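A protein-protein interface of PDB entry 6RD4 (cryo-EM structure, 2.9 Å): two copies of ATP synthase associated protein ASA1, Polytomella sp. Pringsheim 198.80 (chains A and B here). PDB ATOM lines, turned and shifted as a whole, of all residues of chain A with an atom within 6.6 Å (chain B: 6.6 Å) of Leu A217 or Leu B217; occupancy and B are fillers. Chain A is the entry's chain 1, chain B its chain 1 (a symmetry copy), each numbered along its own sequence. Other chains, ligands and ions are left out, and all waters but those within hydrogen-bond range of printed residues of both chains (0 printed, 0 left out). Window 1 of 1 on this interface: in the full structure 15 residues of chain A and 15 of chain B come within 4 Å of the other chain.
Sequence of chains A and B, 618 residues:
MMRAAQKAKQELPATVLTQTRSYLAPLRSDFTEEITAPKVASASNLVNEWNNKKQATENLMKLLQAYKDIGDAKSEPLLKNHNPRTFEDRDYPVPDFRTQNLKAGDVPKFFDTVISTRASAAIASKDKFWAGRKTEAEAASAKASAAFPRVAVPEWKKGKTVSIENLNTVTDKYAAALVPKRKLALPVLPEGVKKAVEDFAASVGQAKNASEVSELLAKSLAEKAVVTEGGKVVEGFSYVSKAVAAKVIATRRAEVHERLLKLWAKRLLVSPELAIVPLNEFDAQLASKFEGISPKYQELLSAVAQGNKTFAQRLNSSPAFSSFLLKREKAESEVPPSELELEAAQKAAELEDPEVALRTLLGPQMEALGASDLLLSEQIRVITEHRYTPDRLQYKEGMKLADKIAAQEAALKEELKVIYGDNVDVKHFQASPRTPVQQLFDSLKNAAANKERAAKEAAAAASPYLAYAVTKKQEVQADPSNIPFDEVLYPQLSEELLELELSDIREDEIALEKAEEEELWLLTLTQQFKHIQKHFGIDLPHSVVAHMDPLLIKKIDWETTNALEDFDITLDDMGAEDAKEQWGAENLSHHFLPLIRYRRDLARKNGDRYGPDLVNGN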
ATOM      1  N   LEU A 189      -5.458  18.026 -16.151  1.00  0.00           N
ATOM      2  CA  LEU A 189      -5.430  17.307 -17.410  1.00  0.00           C
ATOM      3  C   LEU A 189      -4.012  16.816 -17.654  1.00  0.00           C
ATOM      4  O   LEU A 189      -3.098  17.638 -17.772  1.00  0.00           O
ATOM      5  CB  LEU A 189      -5.878  18.203 -18.552  1.00  0.00           C
ATOM      6  CG  LEU A 189      -6.604  17.489 -19.685  1.00  0.00           C
ATOM      7  CD1 LEU A 189      -7.861  16.836 -19.155  1.00  0.00           C
ATOM      8  CD2 LEU A 189      -6.922  18.449 -20.798  1.00  0.00           C
ATOM      9  N   VAL A 193      -3.525  12.881 -22.136  1.00  0.00           N
ATOM     10  CA  VAL A 193      -4.819  13.129 -22.753  1.00  0.00           C
ATOM     11  C   VAL A 193      -4.978  14.572 -23.214  1.00  0.00           C
ATOM     12  O   VAL A 193      -5.904  14.864 -23.983  1.00  0.00           O
ATOM     13  CB  VAL A 193      -5.976  12.735 -21.806  1.00  0.00           C
ATOM     14  CG1 VAL A 193      -6.257  13.821 -20.807  1.00  0.00           C
ATOM     15  CG2 VAL A 193      -7.230  12.295 -22.568  1.00  0.00           C
ATOM     16  N   LYS A 194      -4.108  15.494 -22.805  1.00  0.00           N
ATOM     17  CA  LYS A 194      -4.205  16.833 -23.361  1.00  0.00           C
ATOM     18  C   LYS A 194      -3.535  16.950 -24.715  1.00  0.00           C
ATOM     19  O   LYS A 194      -3.776  17.935 -25.416  1.00  0.00           O
ATOM     20  CB  LYS A 194      -3.623  17.878 -22.412  1.00  0.00           C
ATOM     21  CG  LYS A 194      -2.173  18.233 -22.623  1.00  0.00           C
ATOM     22  CD  LYS A 194      -1.843  19.540 -21.923  1.00  0.00           C
ATOM     23  CE  LYS A 194      -2.365  20.723 -22.695  1.00  0.00           C
ATOM     24  NZ  LYS A 194      -1.724  20.773 -24.027  1.00  0.00           N
ATOM     25  N   VAL A 197      -6.139  15.095 -27.362  1.00  0.00           N
ATOM     26  CA  VAL A 197      -7.223  15.960 -27.806  1.00  0.00           C
ATOM     27  C   VAL A 197      -6.720  17.224 -28.469  1.00  0.00           C
ATOM     28  O   VAL A 197      -7.517  17.922 -29.113  1.00  0.00           O
ATOM     29  CB  VAL A 197      -8.172  16.328 -26.650  1.00  0.00           C
ATOM     30  CG1 VAL A 197      -8.748  15.073 -26.012  1.00  0.00           C
ATOM     31  CG2 VAL A 197      -7.471  17.225 -25.649  1.00  0.00           C
ATOM     32  N   PHE A 200      -5.927  15.869 -32.190  1.00  0.00           N
ATOM     33  CA  PHE A 200      -7.216  15.558 -32.803  1.00  0.00           C
ATOM     34  C   PHE A 200      -7.911  16.813 -33.293  1.00  0.00           C
ATOM     35  O   PHE A 200      -8.690  16.755 -34.248  1.00  0.00           O
ATOM     36  CB  PHE A 200      -8.103  14.829 -31.797  1.00  0.00           C
ATOM     37  CG  PHE A 200      -9.384  14.291 -32.372  1.00  0.00           C
ATOM     38  CD1 PHE A 200      -9.399  13.087 -33.046  1.00  0.00           C
ATOM     39  CD2 PHE A 200     -10.576  14.977 -32.204  1.00  0.00           C
ATOM     40  CE1 PHE A 200     -10.570  12.585 -33.555  1.00  0.00           C
ATOM     41  CE2 PHE A 200     -11.751  14.479 -32.716  1.00  0.00           C
ATOM     42  CZ  PHE A 200     -11.747  13.283 -33.390  1.00  0.00           C
ATOM     43  N   GLU A 212      -7.186  26.687 -26.694  1.00  0.00           N
ATOM     44  CA  GLU A 212      -8.459  26.827 -26.002  1.00  0.00           C
ATOM     45  C   GLU A 212      -9.276  25.546 -26.032  1.00  0.00           C
ATOM     46  O   GLU A 212     -10.152  25.365 -25.185  1.00  0.00           O
ATOM     47  CB  GLU A 212      -9.268  27.990 -26.595  1.00  0.00           C
ATOM     48  CG  GLU A 212      -9.846  27.796 -27.997  1.00  0.00           C
ATOM     49  CD  GLU A 212     -11.281  27.266 -27.994  1.00  0.00           C
ATOM     50  OE1 GLU A 212     -11.954  27.357 -26.948  1.00  0.00           O
ATOM     51  OE2 GLU A 212     -11.740  26.766 -29.039  1.00  0.00           O
ATOM     52  N   VAL A 213      -9.017  24.650 -26.984  1.00  0.00           N
ATOM     53  CA  VAL A 213      -9.838  23.452 -27.091  1.00  0.00           C
ATOM     54  C   VAL A 213      -9.514  22.463 -25.989  1.00  0.00           C
ATOM     55  O   VAL A 213     -10.325  21.579 -25.696  1.00  0.00           O
ATOM     56  CB  VAL A 213      -9.680  22.787 -28.471  1.00  0.00           C
ATOM     57  CG1 VAL A 213     -10.144  23.721 -29.573  1.00  0.00           C
ATOM     58  CG2 VAL A 213      -8.248  22.346 -28.707  1.00  0.00           C
ATOM     59  N   SER A 214      -8.342  22.592 -25.367  1.00  0.00           N
ATOM     60  CA  SER A 214      -7.974  21.734 -24.250  1.00  0.00           C
ATOM     61  C   SER A 214      -8.531  22.265 -22.941  1.00  0.00           C
ATOM     62  O   SER A 214      -8.992  21.488 -22.100  1.00  0.00           O
ATOM     63  CB  SER A 214      -6.455  21.628 -24.164  1.00  0.00           C
ATOM     64  OG  SER A 214      -5.885  22.909 -23.961  1.00  0.00           O
ATOM     65  N   GLU A 215      -8.511  23.590 -22.777  1.00  0.00           N
ATOM     66  CA  GLU A 215      -8.855  24.214 -21.505  1.00  0.00           C
ATOM     67  C   GLU A 215     -10.321  24.024 -21.165  1.00  0.00           C
ATOM     68  O   GLU A 215     -10.676  23.928 -19.988  1.00  0.00           O
ATOM     69  CB  GLU A 215      -8.516  25.700 -21.547  1.00  0.00           C
ATOM     70  CG  GLU A 215      -7.071  25.992 -21.871  1.00  0.00           C
ATOM     71  CD  GLU A 215      -6.882  27.370 -22.457  1.00  0.00           C
ATOM     72  OE1 GLU A 215      -5.734  27.723 -22.791  1.00  0.00           O
ATOM     73  OE2 GLU A 215      -7.883  28.102 -22.581  1.00  0.00           O
ATOM     74  N   LEU A 216     -11.183  23.968 -22.176  1.00  0.00           N
ATOM     75  CA  LEU A 216     -12.593  23.714 -21.921  1.00  0.00           C
ATOM     76  C   LEU A 216     -12.821  22.294 -21.436  1.00  0.00           C
ATOM     77  O   LEU A 216     -13.726  22.053 -20.631  1.00  0.00           O
ATOM     78  CB  LEU A 216     -13.423  23.982 -23.174  1.00  0.00           C
ATOM     79  CG  LEU A 216     -13.949  25.403 -23.400  1.00  0.00           C
ATOM     80  CD1 LEU A 216     -14.825  25.826 -22.230  1.00  0.00           C
ATOM     81  CD2 LEU A 216     -12.860  26.434 -23.654  1.00  0.00           C
ATOM     82  N   LEU A 217     -12.000  21.348 -21.893  1.00  0.00           N
ATOM     83  CA  LEU A 217     -12.089  19.986 -21.383  1.00  0.00           C
ATOM     84  C   LEU A 217     -11.557  19.912 -19.962  1.00  0.00           C
ATOM     85  O   LEU A 217     -12.057  19.135 -19.139  1.00  0.00           O
ATOM     86  CB  LEU A 217     -11.323  19.032 -22.298  1.00  0.00           C
ATOM     87  CG  LEU A 217     -11.432  17.555 -21.928  1.00  0.00           C
ATOM     88  CD1 LEU A 217     -12.885  17.145 -21.824  1.00  0.00           C
ATOM     89  CD2 LEU A 217     -10.711  16.694 -22.930  1.00  0.00           C
ATOM     90  N   ALA A 218     -10.551  20.729 -19.656  1.00  0.00           N
ATOM     91  CA  ALA A 218     -10.048  20.810 -18.294  1.00  0.00           C
ATOM     92  C   ALA A 218     -11.088  21.421 -17.368  1.00  0.00           C
ATOM     93  O   ALA A 218     -11.356  20.892 -16.286  1.00  0.00           O
ATOM     94  CB  ALA A 218      -8.760  21.627 -18.273  1.00  0.00           C
ATOM     95  N   LYS A 219     -11.718  22.517 -17.805  1.00  0.00           N
ATOM     96  CA  LYS A 219     -12.648  23.250 -16.956  1.00  0.00           C
ATOM     97  C   LYS A 219     -13.978  22.536 -16.798  1.00  0.00           C
ATOM     98  O   LYS A 219     -14.663  22.748 -15.799  1.00  0.00           O
ATOM     99  CB  LYS A 219     -12.894  24.640 -17.516  1.00  0.00           C
ATOM    100  CG  LYS A 219     -11.747  25.580 -17.357  1.00  0.00           C
ATOM    101  CD  LYS A 219     -12.197  26.999 -17.588  1.00  0.00           C
ATOM    102  CE  LYS A 219     -11.017  27.948 -17.646  1.00  0.00           C
ATOM    103  NZ  LYS A 219     -10.157  27.681 -18.830  1.00  0.00           N
ATOM    104  N   SER A 220     -14.381  21.720 -17.767  1.00  0.00           N
ATOM    105  CA  SER A 220     -15.672  21.051 -17.642  1.00  0.00           C
ATOM    106  C   SER A 220     -15.632  19.948 -16.596  1.00  0.00           C
ATOM    107  O   SER A 220     -16.655  19.645 -15.981  1.00  0.00           O
ATOM    108  CB  SER A 220     -16.115  20.488 -18.987  1.00  0.00           C
ATOM    109  OG  SER A 220     -17.149  19.538 -18.814  1.00  0.00           O
ATOM    110  N   LEU A 221     -14.470  19.337 -16.390  1.00  0.00           N
ATOM    111  CA  LEU A 221     -14.287  18.440 -15.257  1.00  0.00           C
ATOM    112  C   LEU A 221     -13.973  19.194 -13.979  1.00  0.00           C
ATOM    113  O   LEU A 221     -14.345  18.742 -12.892  1.00  0.00           O
ATOM    114  CB  LEU A 221     -13.172  17.446 -15.548  1.00  0.00           C
ATOM    115  CG  LEU A 221     -13.537  16.248 -16.394  1.00  0.00           C
ATOM    116  CD1 LEU A 221     -12.286  15.529 -16.794  1.00  0.00           C
ATOM    117  CD2 LEU A 221     -14.417  15.352 -15.550  1.00  0.00           C
ATOM    118  N   ALA A 222     -13.300  20.337 -14.090  1.00  0.00           N
ATOM    119  CA  ALA A 222     -12.991  21.136 -12.917  1.00  0.00           C
ATOM    120  C   ALA A 222     -14.246  21.721 -12.299  1.00  0.00           C
ATOM    121  O   ALA A 222     -14.333  21.847 -11.075  1.00  0.00           O
ATOM    122  CB  ALA A 222     -12.027  22.254 -13.289  1.00  0.00           C
ATOM    123  N   LEU B 189     -15.400  12.364 -33.324  1.00  0.00           N
ATOM    124  CA  LEU B 189     -14.467  12.016 -32.270  1.00  0.00           C
ATOM    125  C   LEU B 189     -14.114  10.543 -32.403  1.00  0.00           C
ATOM    126  O   LEU B 189     -15.005   9.695 -32.290  1.00  0.00           O
ATOM    127  CB  LEU B 189     -15.072  12.289 -30.903  1.00  0.00           C
ATOM    128  CG  LEU B 189     -14.075  12.703 -29.828  1.00  0.00           C
ATOM    129  CD1 LEU B 189     -13.386  13.985 -30.237  1.00  0.00           C
ATOM    130  CD2 LEU B 189     -14.764  12.861 -28.500  1.00  0.00           C
ATOM    131  N   VAL B 193      -9.499   8.816 -29.008  1.00  0.00           N
ATOM    132  CA  VAL B 193      -9.468   9.970 -28.122  1.00  0.00           C
ATOM    133  C   VAL B 193     -10.769  10.147 -27.350  1.00  0.00           C
ATOM    134  O   VAL B 193     -10.798  10.914 -26.378  1.00  0.00           O
ATOM    135  CB  VAL B 193      -9.120  11.262 -28.896  1.00  0.00           C
ATOM    136  CG1 VAL B 193     -10.332  11.832 -29.578  1.00  0.00           C
ATOM    137  CG2 VAL B 193      -8.397  12.291 -28.022  1.00  0.00           C
ATOM    138  N   LYS B 194     -11.851   9.459 -27.714  1.00  0.00           N
ATOM    139  CA  LYS B 194     -13.040   9.547 -26.884  1.00  0.00           C
ATOM    140  C   LYS B 194     -12.982   8.623 -25.685  1.00  0.00           C
ATOM    141  O   LYS B 194     -13.782   8.793 -24.762  1.00  0.00           O
ATOM    142  CB  LYS B 194     -14.307   9.263 -27.687  1.00  0.00           C
ATOM    143  CG  LYS B 194     -14.790   7.834 -27.682  1.00  0.00           C
ATOM    144  CD  LYS B 194     -16.235   7.765 -28.144  1.00  0.00           C
ATOM    145  CE  LYS B 194     -17.180   8.210 -27.060  1.00  0.00           C
ATOM    146  NZ  LYS B 194     -17.057   7.312 -25.891  1.00  0.00           N
ATOM    147  N   VAL B 197     -10.362  10.460 -23.041  1.00  0.00           N
ATOM    148  CA  VAL B 197     -10.990  11.495 -22.233  1.00  0.00           C
ATOM    149  C   VAL B 197     -12.159  10.970 -21.427  1.00  0.00           C
ATOM    150  O   VAL B 197     -12.622  11.671 -20.515  1.00  0.00           O
ATOM    151  CB  VAL B 197     -11.450  12.691 -23.089  1.00  0.00           C
ATOM    152  CG1 VAL B 197     -10.276  13.282 -23.854  1.00  0.00           C
ATOM    153  CG2 VAL B 197     -12.597  12.288 -23.994  1.00  0.00           C
ATOM    154  N   PHE B 200     -10.239   9.314 -18.285  1.00  0.00           N
ATOM    155  CA  PHE B 200      -9.664  10.418 -17.520  1.00  0.00           C
ATOM    156  C   PHE B 200     -10.711  11.096 -16.658  1.00  0.00           C
ATOM    157  O   PHE B 200     -10.381  11.652 -15.608  1.00  0.00           O
ATOM    158  CB  PHE B 200      -9.034  11.432 -18.471  1.00  0.00           C
ATOM    159  CG  PHE B 200      -8.247  12.517 -17.791  1.00  0.00           C
ATOM    160  CD1 PHE B 200      -6.945  12.293 -17.391  1.00  0.00           C
ATOM    161  CD2 PHE B 200      -8.802  13.770 -17.587  1.00  0.00           C
ATOM    162  CE1 PHE B 200      -6.218  13.288 -16.788  1.00  0.00           C
ATOM    163  CE2 PHE B 200      -8.077  14.768 -16.979  1.00  0.00           C
ATOM    164  CZ  PHE B 200      -6.786  14.527 -16.581  1.00  0.00           C
ATOM    165  N   GLU B 212     -21.660  12.566 -21.079  1.00  0.00           N
ATOM    166  CA  GLU B 212     -21.771  13.962 -21.476  1.00  0.00           C
ATOM    167  C   GLU B 212     -20.417  14.648 -21.561  1.00  0.00           C
ATOM    168  O   GLU B 212     -20.292  15.662 -22.248  1.00  0.00           O
ATOM    169  CB  GLU B 212     -22.695  14.722 -20.515  1.00  0.00           C
ATOM    170  CG  GLU B 212     -22.174  14.980 -19.100  1.00  0.00           C
ATOM    171  CD  GLU B 212     -21.483  16.335 -18.945  1.00  0.00           C
ATOM    172  OE1 GLU B 212     -21.686  17.216 -19.805  1.00  0.00           O
ATOM    173  OE2 GLU B 212     -20.744  16.525 -17.960  1.00  0.00           O
ATOM    174  N   VAL B 213     -19.396  14.124 -20.881  1.00  0.00           N
ATOM    175  CA  VAL B 213     -18.109  14.804 -20.874  1.00  0.00           C
ATOM    176  C   VAL B 213     -17.390  14.637 -22.198  1.00  0.00           C
ATOM    177  O   VAL B 213     -16.486  15.416 -22.511  1.00  0.00           O
ATOM    178  CB  VAL B 213     -17.222  14.310 -19.716  1.00  0.00           C
ATOM    179  CG1 VAL B 213     -17.870  14.610 -18.377  1.00  0.00           C
ATOM    180  CG2 VAL B 213     -16.922  12.829 -19.850  1.00  0.00           C
ATOM    181  N   SER B 214     -17.776  13.634 -22.988  1.00  0.00           N
ATOM    182  CA  SER B 214     -17.193  13.437 -24.307  1.00  0.00           C
ATOM    183  C   SER B 214     -17.888  14.295 -25.350  1.00  0.00           C
ATOM    184  O   SER B 214     -17.231  14.856 -26.232  1.00  0.00           O
ATOM    185  CB  SER B 214     -17.290  11.965 -24.696  1.00  0.00           C
ATOM    186  OG  SER B 214     -18.646  11.557 -24.732  1.00  0.00           O
ATOM    187  N   GLU B 215     -19.213  14.419 -25.236  1.00  0.00           N
ATOM    188  CA  GLU B 215     -20.017  15.068 -26.263  1.00  0.00           C
ATOM    189  C   GLU B 215     -19.717  16.553 -26.354  1.00  0.00           C
ATOM    190  O   GLU B 215     -19.801  17.135 -27.438  1.00  0.00           O
ATOM    191  CB  GLU B 215     -21.499  14.851 -25.978  1.00  0.00           C
ATOM    192  CG  GLU B 215     -21.899  13.399 -25.877  1.00  0.00           C
ATOM    193  CD  GLU B 215     -23.155  13.205 -25.063  1.00  0.00           C
ATOM    194  OE1 GLU B 215     -23.576  12.046 -24.883  1.00  0.00           O
ATOM    195  OE2 GLU B 215     -23.724  14.215 -24.604  1.00  0.00           O
ATOM    196  N   LEU B 216     -19.368  17.178 -25.234  1.00  0.00           N
ATOM    197  CA  LEU B 216     -18.998  18.585 -25.268  1.00  0.00           C
ATOM    198  C   LEU B 216     -17.676  18.792 -25.986  1.00  0.00           C
ATOM    199  O   LEU B 216     -17.482  19.821 -26.639  1.00  0.00           O
ATOM    200  CB  LEU B 216     -18.923  19.156 -23.854  1.00  0.00           C
ATOM    201  CG  LEU B 216     -20.202  19.738 -23.243  1.00  0.00           C
ATOM    202  CD1 LEU B 216     -20.727  20.869 -24.114  1.00  0.00           C
ATOM    203  CD2 LEU B 216     -21.292  18.708 -22.989  1.00  0.00           C
ATOM    204  N   LEU B 217     -16.768  17.820 -25.897  1.00  0.00           N
ATOM    205  CA  LEU B 217     -15.525  17.901 -26.653  1.00  0.00           C
ATOM    206  C   LEU B 217     -15.784  17.671 -28.132  1.00  0.00           C
ATOM    207  O   LEU B 217     -15.120  18.266 -28.990  1.00  0.00           O
ATOM    208  CB  LEU B 217     -14.517  16.887 -26.116  1.00  0.00           C
ATOM    209  CG  LEU B 217     -13.134  16.949 -26.757  1.00  0.00           C
ATOM    210  CD1 LEU B 217     -12.576  18.354 -26.670  1.00  0.00           C
ATOM    211  CD2 LEU B 217     -12.194  15.968 -26.109  1.00  0.00           C
ATOM    212  N   ALA B 218     -16.760  16.821 -28.445  1.00  0.00           N
ATOM    213  CA  ALA B 218     -17.155  16.621 -29.829  1.00  0.00           C
ATOM    214  C   ALA B 218     -17.797  17.876 -30.397  1.00  0.00           C
ATOM    215  O   ALA B 218     -17.451  18.319 -31.496  1.00  0.00           O
ATOM    216  CB  ALA B 218     -18.111  15.436 -29.921  1.00  0.00           C
ATOM    217  N   LYS B 219     -18.707  18.489 -29.632  1.00  0.00           N
ATOM    218  CA  LYS B 219     -19.467  19.632 -30.121  1.00  0.00           C
ATOM    219  C   LYS B 219     -18.640  20.903 -30.172  1.00  0.00           C
ATOM    220  O   LYS B 219     -18.950  21.796 -30.959  1.00  0.00           O
ATOM    221  CB  LYS B 219     -20.688  19.870 -29.249  1.00  0.00           C
ATOM    222  CG  LYS B 219     -21.773  18.861 -29.421  1.00  0.00           C
ATOM    223  CD  LYS B 219     -23.059  19.367 -28.821  1.00  0.00           C
ATOM    224  CE  LYS B 219     -24.116  18.283 -28.789  1.00  0.00           C
ATOM    225  NZ  LYS B 219     -23.739  17.176 -27.868  1.00  0.00           N
ATOM    226  N   SER B 220     -17.613  21.028 -29.336  1.00  0.00           N
ATOM    227  CA  SER B 220     -16.828  22.257 -29.353  1.00  0.00           C
ATOM    228  C   SER B 220     -15.953  22.346 -30.594  1.00  0.00           C
ATOM    229  O   SER B 220     -15.649  23.446 -31.056  1.00  0.00           O
ATOM    230  CB  SER B 220     -15.974  22.364 -28.096  1.00  0.00           C
ATOM    231  OG  SER B 220     -14.954  23.331 -28.265  1.00  0.00           O
ATOM    232  N   LEU B 221     -15.538  21.206 -31.136  1.00  0.00           N
ATOM    233  CA  LEU B 221     -14.898  21.189 -32.445  1.00  0.00           C
ATOM    234  C   LEU B 221     -15.910  21.211 -33.574  1.00  0.00           C
ATOM    235  O   LEU B 221     -15.627  21.762 -34.641  1.00  0.00           O
ATOM    236  CB  LEU B 221     -14.010  19.961 -32.580  1.00  0.00           C
ATOM    237  CG  LEU B 221     -12.639  20.043 -31.948  1.00  0.00           C
ATOM    238  CD1 LEU B 221     -12.016  18.682 -31.947  1.00  0.00           C
ATOM    239  CD2 LEU B 221     -11.817  21.003 -32.780  1.00  0.00           C
ATOM    240  N   ALA B 222     -17.085  20.625 -33.355  1.00  0.00           N
ATOM    241  CA  ALA B 222     -18.121  20.633 -34.374  1.00  0.00           C
ATOM    242  C   ALA B 222     -18.654  22.032 -34.611  1.00  0.00           C
ATOM    243  O   ALA B 222     -18.995  22.381 -35.744  1.00  0.00           O
ATOM    244  CB  ALA B 222     -19.258  19.707 -33.965  1.00  0.00           C
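Phe B200 touches Leu A189.
Val B197 touches Val A193.
CG1 of Val A193 touches CD1 of Phe B200 (3.8 Å).
Val A197 touches Val B193.
CG1 of Val A197 touches CG1 of Val B197, at 3.2 Å.
CG1 of Val A197 touches CD2 of Leu B217, 3.6 Å away.
Leu B189 touches Phe A200.
Leu B221 touches Phe A200.
Leu A217 touches Val B197.
CD2 of Leu B217 touches CD2 of Leu A217, 3.6 Å away.
Of the printed residues of chain B, Leu A189 touches Phe B200.
Of the printed residues of chain B, Val A193 touches Val B197 and Phe B200.
Of the printed residues of chain B, Val A197 touches Val B193 (3.5 Å), Val B197 (3.2 Å) and Leu B217 (3.6 Å).
Val A213 touches none of the printed residues of chain B.
Printed residues of chain B within 4 Å of Leu A217: Val B197 and Leu B217.
Printed residues of chain A within 4 Å of Phe B200: Leu A189 (3.0 Å), Val A193 (3.8 Å) and Leu A221 (3.98 Å).
Leu B217 touches two residues of chain A.
Ser B220 touches none of the printed residues of chain A.
The nearest residue of chain B that does not touch Leu A217 is Val B213 (4.1 Å).
The nearest residue of chain A that does not touch Leu B217 is Val A213 (4.1 Å).
The nearest printed residue of chain B that does not touch Val A197 is Leu B221 (5.4 Å).
Printed residues of chain B that touch a printed residue of chain A: Leu B189, Val B193, Val B197, Phe B200, Leu B217 and Leu B221.
Among the printed residues, no Asp or Glu carboxylate lies within 4 Å of a Lys or Arg side-chain nitrogen of the other chain.
Leu A189 touches Phe B200, and with the chains exchanged Phe A200 touches Leu B189.
Val A193 touches Phe B200, and with the chains exchanged Phe A200 touches Val B193.
Val A197 touches Leu B217, and with the chains exchanged Leu A217 touches Val B197.
Phe A200 touches Leu B221, and with the chains exchanged Leu A221 touches Phe B200.
Positions printed for both chains: 189, 193, 194, 197, 200, 212, 213, 214, 215, 216, 217, 218, 219, 220, 221 and 222.
Of the 12 pairs that touch across the chains among the printed residues, 12 have their exchanged pair printed and touching as well.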
